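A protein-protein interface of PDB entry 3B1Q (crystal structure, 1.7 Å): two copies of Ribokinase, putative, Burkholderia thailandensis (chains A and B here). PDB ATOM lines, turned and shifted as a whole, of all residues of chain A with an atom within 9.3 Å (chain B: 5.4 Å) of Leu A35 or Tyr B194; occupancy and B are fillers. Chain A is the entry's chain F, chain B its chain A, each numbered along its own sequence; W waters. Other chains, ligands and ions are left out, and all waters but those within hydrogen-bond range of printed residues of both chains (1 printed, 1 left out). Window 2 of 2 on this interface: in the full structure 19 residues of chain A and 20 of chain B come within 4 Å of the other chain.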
ATOM      1  N   ILE A  33      -4.635 -25.004  33.711  1.00  0.00           N
ATOM      2  CA  ILE A  33      -5.006 -23.936  32.780  1.00  0.00           C
ATOM      3  C   ILE A  33      -3.961 -22.802  32.686  1.00  0.00           C
ATOM      4  O   ILE A  33      -3.531 -22.210  33.703  1.00  0.00           O
ATOM      5  CB  ILE A  33      -6.434 -23.343  33.050  1.00  0.00           C
ATOM      6  CG1 ILE A  33      -6.491 -22.568  34.381  1.00  0.00           C
ATOM      7  CG2 ILE A  33      -7.521 -24.435  32.946  1.00  0.00           C
ATOM      8  N   ASN A  34      -3.580 -22.521  31.439  1.00  0.00           N
ATOM      9  CA  ASN A  34      -2.581 -21.516  31.103  1.00  0.00           C
ATOM     10  C   ASN A  34      -3.134 -20.533  30.032  1.00  0.00           C
ATOM     11  O   ASN A  34      -2.732 -20.582  28.861  1.00  0.00           O
ATOM     12  CB  ASN A  34      -1.315 -22.245  30.631  1.00  0.00           C
ATOM     13  CG  ASN A  34      -0.101 -21.341  30.538  1.00  0.00           C
ATOM     14  OD1 ASN A  34      -0.001 -20.322  31.245  1.00  0.00           O
ATOM     15  ND2 ASN A  34       0.847 -21.721  29.665  1.00  0.00           N
ATOM     16  N   LEU A  35      -4.055 -19.673  30.455  1.00  0.00           N
ATOM     17  CA  LEU A  35      -4.842 -18.779  29.566  1.00  0.00           C
ATOM     18  C   LEU A  35      -4.339 -17.331  29.361  1.00  0.00           C
ATOM     19  O   LEU A  35      -4.215 -16.567  30.333  1.00  0.00           O
ATOM     20  CB  LEU A  35      -6.303 -18.699  30.053  1.00  0.00           C
ATOM     21  CG  LEU A  35      -7.149 -19.994  30.175  1.00  0.00           C
ATOM     22  CD1 LEU A  35      -8.622 -19.622  30.374  1.00  0.00           C
ATOM     23  CD2 LEU A  35      -6.978 -20.935  28.995  1.00  0.00           C
ATOM     24  N   SER A  36      -4.098 -16.953  28.097  1.00  0.00           N
ATOM     25  CA  SER A  36      -3.811 -15.538  27.741  1.00  0.00           C
ATOM     26  C   SER A  36      -4.937 -14.874  26.959  1.00  0.00           C
ATOM     27  O   SER A  36      -5.624 -15.512  26.143  1.00  0.00           O
ATOM     28  CB  SER A  36      -2.502 -15.349  26.929  1.00  0.00           C
ATOM     29  OG  SER A  36      -1.512 -16.299  27.246  1.00  0.00           O
ATOM     30  N   PHE A  37      -5.041 -13.579  27.177  1.00  0.00           N
ATOM     31  CA  PHE A  37      -5.969 -12.699  26.488  1.00  0.00           C
ATOM     32  C   PHE A  37      -5.121 -11.648  25.828  1.00  0.00           C
ATOM     33  O   PHE A  37      -4.347 -10.965  26.498  1.00  0.00           O
ATOM     34  CB  PHE A  37      -6.920 -12.065  27.505  1.00  0.00           C
ATOM     35  CG  PHE A  37      -7.746 -13.080  28.218  1.00  0.00           C
ATOM     36  CD1 PHE A  37      -7.777 -13.123  29.610  1.00  0.00           C
ATOM     37  CD2 PHE A  37      -8.482 -14.012  27.488  1.00  0.00           C
ATOM     38  CE1 PHE A  37      -8.567 -14.102  30.271  1.00  0.00           C
ATOM     39  CE2 PHE A  37      -9.279 -14.990  28.127  1.00  0.00           C
ATOM     40  CZ  PHE A  37      -9.320 -15.029  29.522  1.00  0.00           C
ATOM     41  N   LEU A  38      -5.245 -11.539  24.516  1.00  0.00           N
ATOM     42  CA  LEU A  38      -4.550 -10.500  23.786  1.00  0.00           C
ATOM     43  C   LEU A  38      -5.149  -9.135  24.041  1.00  0.00           C
ATOM     44  O   LEU A  38      -6.371  -8.934  23.981  1.00  0.00           O
ATOM     45  CB  LEU A  38      -4.626 -10.821  22.316  1.00  0.00           C
ATOM     46  CG  LEU A  38      -3.412 -10.878  21.421  1.00  0.00           C
ATOM     47  CD1 LEU A  38      -2.252 -11.763  21.901  1.00  0.00           C
ATOM     48  CD2 LEU A  38      -3.961 -11.409  20.132  1.00  0.00           C
ATOM     49  N   GLN B 113      -2.681 -19.963  35.744  1.00  0.00           N
ATOM     50  CA  GLN B 113      -2.309 -18.616  35.347  1.00  0.00           C
ATOM     51  C   GLN B 113      -3.311 -17.949  34.385  1.00  0.00           C
ATOM     52  O   GLN B 113      -3.808 -18.603  33.465  1.00  0.00           O
ATOM     53  CB  GLN B 113      -0.945 -18.647  34.682  1.00  0.00           C
ATOM     54  CG  GLN B 113       0.142 -19.322  35.500  1.00  0.00           C
ATOM     55  CD  GLN B 113       1.540 -19.030  34.980  1.00  0.00           C
ATOM     56  OE1 GLN B 113       2.334 -18.396  35.674  1.00  0.00           O
ATOM     57  NE2 GLN B 113       1.837 -19.452  33.791  1.00  0.00           N
ATOM     58  N   ILE B 114      -3.561 -16.658  34.606  1.00  0.00           N
ATOM     59  CA  ILE B 114      -4.239 -15.796  33.609  1.00  0.00           C
ATOM     60  C   ILE B 114      -3.258 -14.725  33.131  1.00  0.00           C
ATOM     61  O   ILE B 114      -2.664 -14.040  33.957  1.00  0.00           O
ATOM     62  CB  ILE B 114      -5.501 -15.110  34.182  1.00  0.00           C
ATOM     63  CG1 ILE B 114      -6.527 -16.164  34.645  1.00  0.00           C
ATOM     64  CG2 ILE B 114      -6.128 -14.130  33.149  1.00  0.00           C
ATOM     65  CD1 ILE B 114      -7.605 -15.628  35.534  1.00  0.00           C
ATOM     66  N   THR B 115      -3.115 -14.585  31.813  1.00  0.00           N
ATOM     67  CA  THR B 115      -2.190 -13.570  31.255  1.00  0.00           C
ATOM     68  C   THR B 115      -2.932 -12.550  30.385  1.00  0.00           C
ATOM     69  O   THR B 115      -3.754 -12.959  29.561  1.00  0.00           O
ATOM     70  CB  THR B 115      -1.089 -14.250  30.461  1.00  0.00           C
ATOM     71  OG1 THR B 115      -0.334 -15.093  31.349  1.00  0.00           O
ATOM     72  CG2 THR B 115      -0.124 -13.216  29.764  1.00  0.00           C
ATOM     73  N   ASN B 192      -0.156 -28.635  25.706  1.00  0.00           N
ATOM     74  CA  ASN B 192      -0.527 -29.222  27.015  1.00  0.00           C
ATOM     75  C   ASN B 192      -1.848 -30.007  26.947  1.00  0.00           C
ATOM     76  O   ASN B 192      -2.514 -30.071  25.885  1.00  0.00           O
ATOM     77  CB  ASN B 192      -0.503 -28.179  28.156  1.00  0.00           C
ATOM     78  CG  ASN B 192      -1.631 -27.112  28.017  1.00  0.00           C
ATOM     79  OD1 ASN B 192      -2.725 -27.397  27.570  1.00  0.00           O
ATOM     80  ND2 ASN B 192      -1.295 -25.834  28.361  1.00  0.00           N
ATOM     81  N   ASP B 193      -2.215 -30.665  28.042  1.00  0.00           N
ATOM     82  CA  ASP B 193      -3.400 -31.535  27.966  1.00  0.00           C
ATOM     83  C   ASP B 193      -4.746 -30.768  27.718  1.00  0.00           C
ATOM     84  O   ASP B 193      -5.615 -31.239  26.986  1.00  0.00           O
ATOM     85  CB  ASP B 193      -3.432 -32.540  29.129  1.00  0.00           C
ATOM     86  CG  ASP B 193      -3.309 -31.887  30.509  1.00  0.00           C
ATOM     87  OD1 ASP B 193      -3.251 -30.660  30.618  1.00  0.00           O
ATOM     88  OD2 ASP B 193      -3.277 -32.635  31.512  1.00  0.00           O
ATOM     89  N   TYR B 194      -4.840 -29.551  28.249  1.00  0.00           N
ATOM     90  CA  TYR B 194      -6.015 -28.713  28.019  1.00  0.00           C
ATOM     91  C   TYR B 194      -6.095 -28.322  26.515  1.00  0.00           C
ATOM     92  O   TYR B 194      -7.160 -28.454  25.859  1.00  0.00           O
ATOM     93  CB  TYR B 194      -5.876 -27.454  28.893  1.00  0.00           C
ATOM     94  CG  TYR B 194      -7.046 -26.514  28.713  1.00  0.00           C
ATOM     95  CD1 TYR B 194      -6.891 -25.290  28.060  1.00  0.00           C
ATOM     96  CD2 TYR B 194      -8.299 -26.856  29.198  1.00  0.00           C
ATOM     97  CE1 TYR B 194      -7.984 -24.432  27.891  1.00  0.00           C
ATOM     98  CE2 TYR B 194      -9.386 -26.018  29.017  1.00  0.00           C
ATOM     99  CZ  TYR B 194      -9.207 -24.803  28.368  1.00  0.00           C
ATOM    100  OH  TYR B 194     -10.289 -23.967  28.203  1.00  0.00           O
ATOM    101  N   GLU B 195      -4.941 -27.948  25.967  1.00  0.00           N
ATOM    102  CA  GLU B 195      -4.807 -27.553  24.576  1.00  0.00           C
ATOM    103  C   GLU B 195      -5.055 -28.731  23.663  1.00  0.00           C
ATOM    104  O   GLU B 195      -5.653 -28.543  22.618  1.00  0.00           O
ATOM    105  CB  GLU B 195      -3.428 -26.975  24.275  1.00  0.00           C
ATOM    106  CG  GLU B 195      -3.255 -25.545  24.797  1.00  0.00           C
ATOM    107  CD  GLU B 195      -1.777 -25.138  24.961  1.00  0.00           C
ATOM    108  OE1 GLU B 195      -0.828 -25.951  24.752  1.00  0.00           O
ATOM    109  OE2 GLU B 195      -1.564 -23.948  25.297  1.00  0.00           O
ATOM    110  N   ALA B 196      -4.604 -29.932  24.046  1.00  0.00           N
ATOM    111  CA  ALA B 196      -4.905 -31.134  23.215  1.00  0.00           C
ATOM    112  C   ALA B 196      -6.426 -31.297  23.025  1.00  0.00           C
ATOM    113  O   ALA B 196      -6.902 -31.611  21.941  1.00  0.00           O
ATOM    114  CB  ALA B 196      -4.310 -32.445  23.839  1.00  0.00           C
ATOM    115  N   LYS B 197      -7.204 -31.097  24.086  1.00  0.00           N
ATOM    116  CA  LYS B 197      -8.649 -31.187  23.926  1.00  0.00           C
ATOM    117  C   LYS B 197      -9.231 -30.101  22.982  1.00  0.00           C
ATOM    118  O   LYS B 197     -10.108 -30.379  22.146  1.00  0.00           O
ATOM    119  CB  LYS B 197      -9.337 -31.097  25.297  1.00  0.00           C
ATOM    120  CG  LYS B 197     -10.869 -31.152  25.184  1.00  0.00           C
ATOM    121  CD  LYS B 197     -11.412 -32.437  24.576  1.00  0.00           C
ATOM    122  CE  LYS B 197     -12.975 -32.486  24.779  1.00  0.00           C
ATOM    123  NZ  LYS B 197     -13.617 -33.358  23.779  1.00  0.00           N
ATOM    124  N   LEU B 198      -8.782 -28.859  23.193  1.00  0.00           N
ATOM    125  CA  LEU B 198      -9.167 -27.757  22.328  1.00  0.00           C
ATOM    126  C   LEU B 198      -8.851 -28.051  20.872  1.00  0.00           C
ATOM    127  O   LEU B 198      -9.684 -27.831  20.018  1.00  0.00           O
ATOM    128  CB  LEU B 198      -8.495 -26.462  22.728  1.00  0.00           C
ATOM    129  CG  LEU B 198      -8.891 -25.949  24.118  1.00  0.00           C
ATOM    130  CD1 LEU B 198      -8.152 -24.636  24.385  1.00  0.00           C
ATOM    131  CD2 LEU B 198     -10.379 -25.775  24.240  1.00  0.00           C
ATOM    132  N   VAL B 199      -7.653 -28.571  20.619  1.00  0.00           N
ATOM    133  CA  VAL B 199      -7.251 -28.971  19.244  1.00  0.00           C
ATOM    134  C   VAL B 199      -8.143 -30.083  18.670  1.00  0.00           C
ATOM    135  O   VAL B 199      -8.644 -29.981  17.500  1.00  0.00           O
ATOM    136  CB  VAL B 199      -5.698 -29.324  19.177  1.00  0.00           C
ATOM    137  CG1 VAL B 199      -5.364 -29.812  17.735  1.00  0.00           C
ATOM    138  CG2 VAL B 199      -4.834 -28.101  19.443  1.00  0.00           C
HETATM  139  O   HOH W   1       3.095 -18.821  31.348  1.00  0.00           O
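N of Thr B115 sits at hydrogen-bond distance from O of Leu A35.
The side-chain amide nitrogen (NE2) of Gln B113 is in hydrogen-bond range of the side-chain amide oxygen (OD1) of Asn A34.
The backbone NH (N) of Leu A35 lies within hydrogen-bond range of the backbone carbonyl oxygen (O) of Gln B113 (3.2 Å).
The backbone carbonyl oxygen (O) of Ile A33 lies within hydrogen-bond range of the backbone NH (N) of Gln B113.
O of Thr B115 lies within hydrogen-bond range of N of Phe A37 (2.8 Å).
The side-chain amide oxygen of Asn B192 sits at hydrogen-bond distance from the backbone NH of Tyr B194.
CA of Ile B114 touches O of Leu A35, at 3.4 Å.
Leu A35 touches Tyr B194.
CA of Ser A36 touches O of Thr B115, at 3.2 Å.
Ile B114 touches Phe A37 (CG2 to CE1, 3.8 Å).
Of the printed residues of chain B, Ile A33 touches Gln B113 (3.2 Å).
Of chain B, only Gln B113 (3.2 Å), Ile B114 (3.4 Å), Thr B115 (2.7 Å) and Tyr B194 (3.8 Å) come within 4 Å of Leu A35.
Printed residues of chain B within 4 Å of Phe A37: Ile B114 (3.8 Å) and Thr B115 (2.8 Å).
Of the printed residues of chain A, Thr B115 touches Leu A35 (2.7 Å), Ser A36 (3.2 Å) and Phe A37 (2.8 Å).
Asn B192 touches none of the printed residues of chain A.
No residue of chain A comes within 4 Å of Ala B196.
Leu B198 touches none of the printed residues of chain A.
The nearest printed residue of chain B that does not touch Leu A35 is Leu B198 (6.0 Å).
Of the 11 printed residues of chain B, 4 touch a printed residue of chain A.
No position is printed for both chains.
Water W1 bridges the side-chain amide nitrogen (NE2) of Gln B113 (2.8 Å) and the side-chain amide oxygen (OD1) of Asn A34 (3.4 Å).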
